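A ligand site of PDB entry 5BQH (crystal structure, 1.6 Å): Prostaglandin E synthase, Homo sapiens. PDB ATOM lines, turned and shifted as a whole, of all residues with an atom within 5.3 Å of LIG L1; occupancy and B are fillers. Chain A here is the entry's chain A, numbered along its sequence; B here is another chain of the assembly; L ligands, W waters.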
ATOM      1  N   ARG A  72     -25.166  -1.860   3.909  1.00  0.00           N
ATOM      2  CA  ARG A  72     -25.697  -3.224   3.784  1.00  0.00           C
ATOM      3  C   ARG A  72     -25.027  -4.192   4.748  1.00  0.00           C
ATOM      4  O   ARG A  72     -25.701  -5.037   5.352  1.00  0.00           O
ATOM      5  CB  ARG A  72     -25.579  -3.743   2.341  1.00  0.00           C
ATOM      6  CG  ARG A  72     -26.536  -3.098   1.352  1.00  0.00           C
ATOM      7  CD  ARG A  72     -26.638  -3.877   0.051  1.00  0.00           C
ATOM      8  NE  ARG A  72     -25.383  -3.958  -0.707  1.00  0.00           N
ATOM      9  CZ  ARG A  72     -24.900  -2.984  -1.480  1.00  0.00           C
ATOM     10  NH1 ARG A  72     -25.563  -1.844  -1.630  1.00  0.00           N
ATOM     11  NH2 ARG A  72     -23.750  -3.157  -2.119  1.00  0.00           N
ATOM     12  N   ALA A  73     -23.712  -4.083   4.895  1.00  0.00           N
ATOM     13  CA  ALA A  73     -22.970  -4.937   5.840  1.00  0.00           C
ATOM     14  C   ALA A  73     -23.453  -4.692   7.262  1.00  0.00           C
ATOM     15  O   ALA A  73     -23.701  -5.640   8.008  1.00  0.00           O
ATOM     16  CB  ALA A  73     -21.473  -4.701   5.723  1.00  0.00           C
ATOM     17  N   ARG A  75     -26.355  -3.397   8.177  1.00  0.00           N
ATOM     18  CA  ARG A  75     -27.724  -3.883   8.314  1.00  0.00           C
ATOM     19  C   ARG A  75     -27.760  -5.408   8.475  1.00  0.00           C
ATOM     20  O   ARG A  75     -28.497  -5.914   9.313  1.00  0.00           O
ATOM     21  CB  ARG A  75     -28.609  -3.433   7.165  1.00  0.00           C
ATOM     22  CG  ARG A  75     -30.065  -3.807   7.392  1.00  0.00           C
ATOM     23  CD  ARG A  75     -30.980  -3.367   6.274  1.00  0.00           C
ATOM     24  NE  ARG A  75     -32.206  -4.151   6.299  1.00  0.00           N
ATOM     25  CZ  ARG A  75     -33.392  -3.735   5.850  1.00  0.00           C
ATOM     26  NH1 ARG A  75     -34.439  -4.546   5.926  1.00  0.00           N
ATOM     27  NH2 ARG A  75     -33.539  -2.526   5.319  1.00  0.00           N
ATOM     28  N   ASN A  76     -26.967  -6.117   7.688  1.00  0.00           N
ATOM     29  CA  ASN A  76     -26.924  -7.567   7.832  1.00  0.00           C
ATOM     30  C   ASN A  76     -26.446  -7.977   9.228  1.00  0.00           C
ATOM     31  O   ASN A  76     -26.984  -8.920   9.821  1.00  0.00           O
ATOM     32  CB  ASN A  76     -26.095  -8.231   6.722  1.00  0.00           C
ATOM     33  CG  ASN A  76     -26.306  -9.723   6.668  1.00  0.00           C
ATOM     34  OD1 ASN A  76     -25.644 -10.482   7.364  1.00  0.00           O
ATOM     35  ND2 ASN A  76     -27.257 -10.163   5.849  1.00  0.00           N
ATOM     36  N   GLU A  79     -29.328  -7.711  11.512  1.00  0.00           N
ATOM     37  CA  GLU A  79     -30.272  -8.800  11.246  1.00  0.00           C
ATOM     38  C   GLU A  79     -29.836 -10.120  11.870  1.00  0.00           C
ATOM     39  O   GLU A  79     -30.663 -11.020  12.043  1.00  0.00           O
ATOM     40  CB  GLU A  79     -30.498  -8.963   9.726  1.00  0.00           C
ATOM     41  CG  GLU A  79     -31.233  -7.771   9.077  1.00  0.00           C
ATOM     42  CD  GLU A  79     -31.243  -7.799   7.548  1.00  0.00           C
ATOM     43  OE1 GLU A  79     -30.632  -8.696   6.942  1.00  0.00           O
ATOM     44  OE2 GLU A  79     -31.860  -6.899   6.945  1.00  0.00           O
ATOM     45  N   HIS A 115     -17.930 -12.857   7.216  1.00  0.00           N
ATOM     46  CA  HIS A 115     -18.985 -12.170   6.473  1.00  0.00           C
ATOM     47  C   HIS A 115     -18.641 -10.708   6.183  1.00  0.00           C
ATOM     48  O   HIS A 115     -18.760 -10.250   5.046  1.00  0.00           O
ATOM     49  CB  HIS A 115     -20.329 -12.254   7.218  1.00  0.00           C
ATOM     50  CG  HIS A 115     -21.498 -11.737   6.418  1.00  0.00           C
ATOM     51  ND1 HIS A 115     -21.852 -10.400   6.400  1.00  0.00           N
ATOM     52  CD2 HIS A 115     -22.386 -12.377   5.635  1.00  0.00           C
ATOM     53  CE1 HIS A 115     -22.912 -10.245   5.626  1.00  0.00           C
ATOM     54  NE2 HIS A 115     -23.256 -11.431   5.138  1.00  0.00           N
ATOM     55  N   TYR A 119     -17.893  -9.075   2.641  1.00  0.00           N
ATOM     56  CA  TYR A 119     -18.769  -8.011   2.154  1.00  0.00           C
ATOM     57  C   TYR A 119     -17.988  -6.752   1.772  1.00  0.00           C
ATOM     58  O   TYR A 119     -18.094  -6.269   0.646  1.00  0.00           O
ATOM     59  CB  TYR A 119     -19.839  -7.639   3.194  1.00  0.00           C
ATOM     60  CG  TYR A 119     -21.192  -7.343   2.573  1.00  0.00           C
ATOM     61  CD1 TYR A 119     -21.307  -6.969   1.232  1.00  0.00           C
ATOM     62  CD2 TYR A 119     -22.361  -7.437   3.333  1.00  0.00           C
ATOM     63  CE1 TYR A 119     -22.534  -6.719   0.657  1.00  0.00           C
ATOM     64  CE2 TYR A 119     -23.610  -7.188   2.759  1.00  0.00           C
ATOM     65  CZ  TYR A 119     -23.688  -6.832   1.419  1.00  0.00           C
ATOM     66  OH  TYR A 119     -24.898  -6.581   0.821  1.00  0.00           O
ATOM     67  N   ARG A 128     -19.522 -14.659   0.626  1.00  0.00           N
ATOM     68  CA  ARG A 128     -20.321 -13.968   1.637  1.00  0.00           C
ATOM     69  C   ARG A 128     -21.574 -14.764   2.010  1.00  0.00           C
ATOM     70  O   ARG A 128     -21.888 -14.925   3.204  1.00  0.00           O
ATOM     71  CB  ARG A 128     -20.709 -12.569   1.165  1.00  0.00           C
ATOM     72  CG  ARG A 128     -21.344 -11.705   2.252  1.00  0.00           C
ATOM     73  CD  ARG A 128     -22.137 -10.554   1.655  1.00  0.00           C
ATOM     74  NE  ARG A 128     -23.367 -10.999   1.009  1.00  0.00           N
ATOM     75  CZ  ARG A 128     -23.563 -11.043  -0.316  1.00  0.00           C
ATOM     76  NH1 ARG A 128     -22.604 -10.666  -1.165  1.00  0.00           N
ATOM     77  NH2 ARG A 128     -24.722 -11.476  -0.788  1.00  0.00           N
ATOM     78  N   SER A 129     -22.289 -15.266   1.001  1.00  0.00           N
ATOM     79  CA  SER A 129     -23.506 -16.026   1.245  1.00  0.00           C
ATOM     80  C   SER A 129     -23.243 -17.264   2.107  1.00  0.00           C
ATOM     81  O   SER A 129     -24.019 -17.557   3.023  1.00  0.00           O
ATOM     82  CB  SER A 129     -24.171 -16.417  -0.091  1.00  0.00           C
ATOM     83  OG  SER A 129     -25.483 -16.876   0.141  1.00  0.00           O
ATOM     84  N   TYR A 132     -22.682 -16.297   5.768  1.00  0.00           N
ATOM     85  CA  TYR A 132     -23.980 -15.981   6.383  1.00  0.00           C
ATOM     86  C   TYR A 132     -24.651 -17.275   6.861  1.00  0.00           C
ATOM     87  O   TYR A 132     -25.093 -17.361   7.999  1.00  0.00           O
ATOM     88  CB  TYR A 132     -24.901 -15.247   5.398  1.00  0.00           C
ATOM     89  CG  TYR A 132     -26.345 -15.176   5.858  1.00  0.00           C
ATOM     90  CD1 TYR A 132     -26.759 -14.188   6.754  1.00  0.00           C
ATOM     91  CD2 TYR A 132     -27.285 -16.112   5.418  1.00  0.00           C
ATOM     92  CE1 TYR A 132     -28.078 -14.121   7.191  1.00  0.00           C
ATOM     93  CE2 TYR A 132     -28.607 -16.058   5.862  1.00  0.00           C
ATOM     94  CZ  TYR A 132     -28.991 -15.063   6.736  1.00  0.00           C
ATOM     95  OH  TYR A 132     -30.306 -15.009   7.168  1.00  0.00           O
ATOM     96  N   ALA B  33     -35.885 -13.459   6.386  1.00  0.00           N
ATOM     97  CA  ALA B  33     -34.579 -13.427   5.697  1.00  0.00           C
ATOM     98  C   ALA B  33     -34.495 -14.474   4.591  1.00  0.00           C
ATOM     99  O   ALA B  33     -34.028 -14.178   3.491  1.00  0.00           O
ATOM    100  CB  ALA B  33     -33.435 -13.599   6.699  1.00  0.00           C
ATOM    101  N   THR B  36     -36.674 -13.406   1.685  1.00  0.00           N
ATOM    102  CA  THR B  36     -35.988 -12.335   0.952  1.00  0.00           C
ATOM    103  C   THR B  36     -34.976 -12.911  -0.045  1.00  0.00           C
ATOM    104  O   THR B  36     -34.940 -12.497  -1.202  1.00  0.00           O
ATOM    105  CB  THR B  36     -35.273 -11.350   1.914  1.00  0.00           C
ATOM    106  OG1 THR B  36     -36.214 -10.860   2.889  1.00  0.00           O
ATOM    107  CG2 THR B  36     -34.689 -10.178   1.146  1.00  0.00           C
ATOM    108  N   GLY B  37     -34.162 -13.860   0.411  1.00  0.00           N
ATOM    109  CA  GLY B  37     -33.160 -14.503  -0.439  1.00  0.00           C
ATOM    110  C   GLY B  37     -33.800 -15.208  -1.622  1.00  0.00           C
ATOM    111  O   GLY B  37     -33.309 -15.114  -2.750  1.00  0.00           O
ATOM    112  N   ARG B  40     -34.952 -12.683  -4.156  1.00  0.00           N
ATOM    113  CA  ARG B  40     -33.780 -12.192  -4.903  1.00  0.00           C
ATOM    114  C   ARG B  40     -33.364 -13.154  -6.007  1.00  0.00           C
ATOM    115  O   ARG B  40     -33.098 -12.735  -7.136  1.00  0.00           O
ATOM    116  CB  ARG B  40     -32.596 -11.940  -3.966  1.00  0.00           C
ATOM    117  CG  ARG B  40     -32.728 -10.710  -3.070  1.00  0.00           C
ATOM    118  CD  ARG B  40     -31.370 -10.372  -2.492  1.00  0.00           C
ATOM    119  NE  ARG B  40     -31.384  -9.193  -1.617  1.00  0.00           N
ATOM    120  CZ  ARG B  40     -31.362  -7.933  -2.040  1.00  0.00           C
ATOM    121  NH1 ARG B  40     -31.358  -7.647  -3.341  1.00  0.00           N
ATOM    122  NH2 ARG B  40     -31.360  -6.945  -1.154  1.00  0.00           N
ATOM    123  N   ALA B  47     -28.322  -7.156  -4.702  1.00  0.00           N
ATOM    124  CA  ALA B  47     -27.839  -5.880  -4.194  1.00  0.00           C
ATOM    125  C   ALA B  47     -26.364  -5.619  -4.518  1.00  0.00           C
ATOM    126  O   ALA B  47     -25.896  -4.488  -4.416  1.00  0.00           O
ATOM    127  CB  ALA B  47     -28.076  -5.793  -2.685  1.00  0.00           C
ATOM    128  N   ASN B  48     -25.652  -6.675  -4.917  1.00  0.00           N
ATOM    129  CA  ASN B  48     -24.209  -6.601  -5.124  1.00  0.00           C
ATOM    130  C   ASN B  48     -23.799  -7.091  -6.499  1.00  0.00           C
ATOM    131  O   ASN B  48     -24.312  -8.112  -6.954  1.00  0.00           O
ATOM    132  CB  ASN B  48     -23.481  -7.423  -4.066  1.00  0.00           C
ATOM    133  CG  ASN B  48     -23.867  -7.025  -2.669  1.00  0.00           C
ATOM    134  OD1 ASN B  48     -23.537  -5.933  -2.223  1.00  0.00           O
ATOM    135  ND2 ASN B  48     -24.584  -7.898  -1.976  1.00  0.00           N
ATOM    136  N   VAL B  67     -38.536  -7.455  -3.416  1.00  0.00           N
ATOM    137  CA  VAL B  67     -37.357  -7.481  -2.549  1.00  0.00           C
ATOM    138  C   VAL B  67     -37.410  -6.305  -1.562  1.00  0.00           C
ATOM    139  O   VAL B  67     -37.205  -6.501  -0.358  1.00  0.00           O
ATOM    140  CB  VAL B  67     -36.025  -7.455  -3.342  1.00  0.00           C
ATOM    141  CG1 VAL B  67     -34.835  -7.448  -2.395  1.00  0.00           C
ATOM    142  CG2 VAL B  67     -35.932  -8.650  -4.273  1.00  0.00           C
ATOM    143  N   LEU B  71     -37.528  -6.363   2.567  1.00  0.00           N
ATOM    144  CA  LEU B  71     -36.610  -5.586   3.387  1.00  0.00           C
ATOM    145  C   LEU B  71     -37.343  -4.674   4.361  1.00  0.00           C
ATOM    146  O   LEU B  71     -36.928  -4.522   5.509  1.00  0.00           O
ATOM    147  CB  LEU B  71     -35.613  -4.794   2.526  1.00  0.00           C
ATOM    148  CG  LEU B  71     -34.504  -5.607   1.844  1.00  0.00           C
ATOM    149  CD1 LEU B  71     -33.756  -4.727   0.865  1.00  0.00           C
ATOM    150  CD2 LEU B  71     -33.548  -6.216   2.860  1.00  0.00           C
ATOM    151  N   HIS B  74     -38.717  -6.843   7.214  1.00  0.00           N
ATOM    152  CA  HIS B  74     -37.607  -7.220   8.092  1.00  0.00           C
ATOM    153  C   HIS B  74     -37.169  -6.030   8.948  1.00  0.00           C
ATOM    154  O   HIS B  74     -36.926  -6.183  10.148  1.00  0.00           O
ATOM    155  CB  HIS B  74     -36.426  -7.759   7.264  1.00  0.00           C
ATOM    156  CG  HIS B  74     -35.488  -8.649   8.034  1.00  0.00           C
ATOM    157  ND1 HIS B  74     -34.574  -9.463   7.411  1.00  0.00           N
ATOM    158  CD2 HIS B  74     -35.331  -8.849   9.362  1.00  0.00           C
ATOM    159  CE1 HIS B  74     -33.889 -10.131   8.322  1.00  0.00           C
ATOM    160  NE2 HIS B  74     -34.331  -9.777   9.516  1.00  0.00           N
HETATM  161  N1  LIG L   1     -31.723  -8.816   4.111  1.00  0.00           N
HETATM  162  C1  LIG L   1     -30.990  -9.926   3.444  1.00  0.00           C
HETATM  163  C2  LIG L   1     -30.795  -9.659   1.966  1.00  0.00           C
HETATM  164  O1  LIG L   1     -29.965 -10.347   1.340  1.00  0.00           O
HETATM  165  O2  LIG L   1     -31.437  -8.745   1.416  1.00  0.00           O
HETATM  166  C3  LIG L   1     -31.733 -11.243   3.719  1.00  0.00           C
HETATM  167  C4  LIG L   1     -30.972 -12.517   3.328  1.00  0.00           C
HETATM  168  C5  LIG L   1     -29.529 -12.504   3.786  1.00  0.00           C
HETATM  169  O3  LIG L   1     -29.225 -12.150   4.924  1.00  0.00           O
HETATM  170  N2  LIG L   1     -28.616 -12.899   2.901  1.00  0.00           N
HETATM  171  C6  LIG L   1     -27.196 -12.927   3.198  1.00  0.00           C
HETATM  172  C7  LIG L   1     -26.474 -11.631   2.915  1.00  0.00           C
HETATM  173  O4  LIG L   1     -25.281 -11.538   3.131  1.00  0.00           O
HETATM  174  C8  LIG L   1     -26.534 -14.065   2.425  1.00  0.00           C
HETATM  175  S1  LIG L   1     -26.717 -13.889   0.638  1.00  0.00           S
HETATM  176  N3  LIG L   1     -27.217 -10.621   2.427  1.00  0.00           N
HETATM  177  C9  LIG L   1     -26.632  -9.365   1.971  1.00  0.00           C
HETATM  178  C10 LIG L   1     -27.304  -8.169   2.617  1.00  0.00           C
HETATM  179  O5  LIG L   1     -28.075  -8.364   3.577  1.00  0.00           O
HETATM  180  O6  LIG L   1     -27.048  -7.031   2.177  1.00  0.00           O
HETATM  181  O1  LG2 L   2     -31.106 -17.157  -0.078  1.00  0.00           O
HETATM  182  C1  LG2 L   2     -23.819 -22.924   2.552  1.00  0.00           C
HETATM  183  C2  LG2 L   2     -23.298 -24.163   2.250  1.00  0.00           C
HETATM  184  C3  LG2 L   2     -24.245 -21.667  -2.270  1.00  0.00           C
HETATM  185  N1  LG2 L   2     -24.736 -20.563  -2.911  1.00  0.00           N
HETATM  186  C4  LG2 L   2     -23.127 -24.574   0.940  1.00  0.00           C
HETATM  187  C5  LG2 L   2     -23.479 -23.713  -0.085  1.00  0.00           C
HETATM  188  C6  LG2 L   2     -24.011 -22.458   0.192  1.00  0.00           C
HETATM  189  C7  LG2 L   2     -24.383 -21.544  -0.907  1.00  0.00           C
HETATM  190  F1  LG2 L   2     -23.703 -15.313  -3.489  1.00  0.00           F
HETATM  191  C8  LG2 L   2     -24.706 -15.484  -4.403  1.00  0.00           C
HETATM  192  F2  LG2 L   2     -24.568 -14.501  -5.333  1.00  0.00           F
HETATM  193  C9  LG2 L   2     -26.052 -15.413  -3.686  1.00  0.00           C
HETATM  194  C10 LG2 L   2     -26.723 -14.202  -3.540  1.00  0.00           C
HETATM  195  C11 LG2 L   2     -27.947 -14.135  -2.900  1.00  0.00           C
HETATM  196  C12 LG2 L   2     -28.544 -15.274  -2.368  1.00  0.00           C
HETATM  197  C13 LG2 L   2     -29.872 -15.209  -1.656  1.00  0.00           C
HETATM  198  N2  LG2 L   2     -29.724 -15.390  -0.220  1.00  0.00           N
HETATM  199  C14 LG2 L   2     -30.286 -16.408   0.441  1.00  0.00           C
HETATM  200  C15 LG2 L   2     -29.861 -16.564   1.889  1.00  0.00           C
HETATM  201  C16 LG2 L   2     -29.175 -17.908   2.099  1.00  0.00           C
HETATM  202  C17 LG2 L   2     -31.063 -16.404   2.822  1.00  0.00           C
HETATM  203  C18 LG2 L   2     -27.887 -16.490  -2.516  1.00  0.00           C
HETATM  204  C19 LG2 L   2     -26.649 -16.572  -3.164  1.00  0.00           C
HETATM  205  C20 LG2 L   2     -25.989 -17.902  -3.298  1.00  0.00           C
HETATM  206  O2  LG2 L   2     -25.701 -18.377  -4.392  1.00  0.00           O
HETATM  207  N3  LG2 L   2     -25.753 -18.571  -2.111  1.00  0.00           N
HETATM  208  C21 LG2 L   2     -25.169 -19.793  -1.926  1.00  0.00           C
HETATM  209  N4  LG2 L   2     -24.983 -20.334  -0.700  1.00  0.00           N
HETATM  210  C22 LG2 L   2     -24.179 -22.080   1.520  1.00  0.00           C
HETATM  211 CL1  LG2 L   2     -22.852 -25.241   3.544  1.00  0.00          CL
HETATM  212  O   HOH W   1     -28.467 -11.296  -0.742  1.00  0.00           O
HETATM  213  O   HOH W   2     -30.557 -11.364   7.260  1.00  0.00           O
HETATM  214  O   HOH W   3     -34.384  -9.290   4.614  1.00  0.00           O
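OH of Tyr 119 sits at hydrogen-bond distance from O6 of LIG L1 (2.6 Å).
A ring nitrogen (NE2) of His 115 lies within hydrogen-bond range of an oxygen (O4) of LIG L1 (2.9 Å).
The guanidinium group (NE) of Arg 128 sits at hydrogen-bond distance from an oxygen (O4) of LIG L1, at 2.9 Å.
ND2 of Asn 76 is in hydrogen-bond range of O3 of LIG L1.
OE1 of Glu 79 is in salt-bridge range of N1 of LIG L1.
The guanidinium group (NE) of Arg 40 of chain B lies within salt-bridge range of an oxygen (O2) of LIG L1, 3.1 Å away.
A sulfur (S1) of LIG L1 lies close to the side-chain hydroxyl (OG) of Ser 129 (3.3 Å).
A nitrogen (N3) of LG2 L2 sits at hydrogen-bond distance from the side-chain hydroxyl (OG) of Ser 129 (2.8 Å).
Merely in contact with LIG L1: Arg 72 (3.6 Å), Tyr 132 (3.2 Å), Ala 33 of chain B (3.5 Å), Thr 36 of chain B (3.6 Å) and Leu 71 of chain B (3.4 Å).
Hydrophobic or aromatic side chains that line LIG L1: His 115, Tyr 119, Tyr 132 and Leu 71 of chain B.
Of the 19 residues printed, 12 come within 4 Å of LIG L1.
Along chain A the residues within 4 Å of LIG L1 span positions 72 to 132.
The nearest printed residue that does not touch LIG L1 is His 74 of chain B (4.4 Å).
The side-chain hydroxyl (OH) of Tyr 119 lies within hydrogen-bond range of the guanidinium group (NE) of Arg 72, 3.1 Å away.
ND2 of Asn 48 of chain B lies within hydrogen-bond range of OH of Tyr 119.
NE2 of His 115 sits close to OD1 of Asn 76, 3.4 Å away.
The guanidinium group (NH1) of Arg 128 sits close to the side-chain amide nitrogen (ND2) of Asn 48 of chain B (3.5 Å).
NE of Arg 75 lies within salt-bridge range of OE2 of Glu 79.
The backbone carbonyl oxygen (O) of Leu 71 of chain B is in hydrogen-bond range of the guanidinium group (NH1) of Arg 75 (2.5 Å).
NH2 of Arg 72 lies within hydrogen-bond range of OD1 of Asn 48 of chain B, 2.8 Å away.
The guanidinium group of Arg 72 is in hydrogen-bond range of the backbone carbonyl oxygen of Ala 47 of chain B (3.4 Å).
A sulfur (S1) of LIG L1 sits close to a nitrogen (N2) of LG2 L2, at 3.5 Å.
Water W3 lies within hydrogen-bond range of N1 of LIG L1 (2.7 Å), ND1 of His 74 of chain B (2.8 Å) and OG1 of Thr 36 of chain B (3.0 Å).
Water W2 bridges OE1 of Glu 79 (2.7 Å) and O3 of LIG L1 (2.8 Å).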
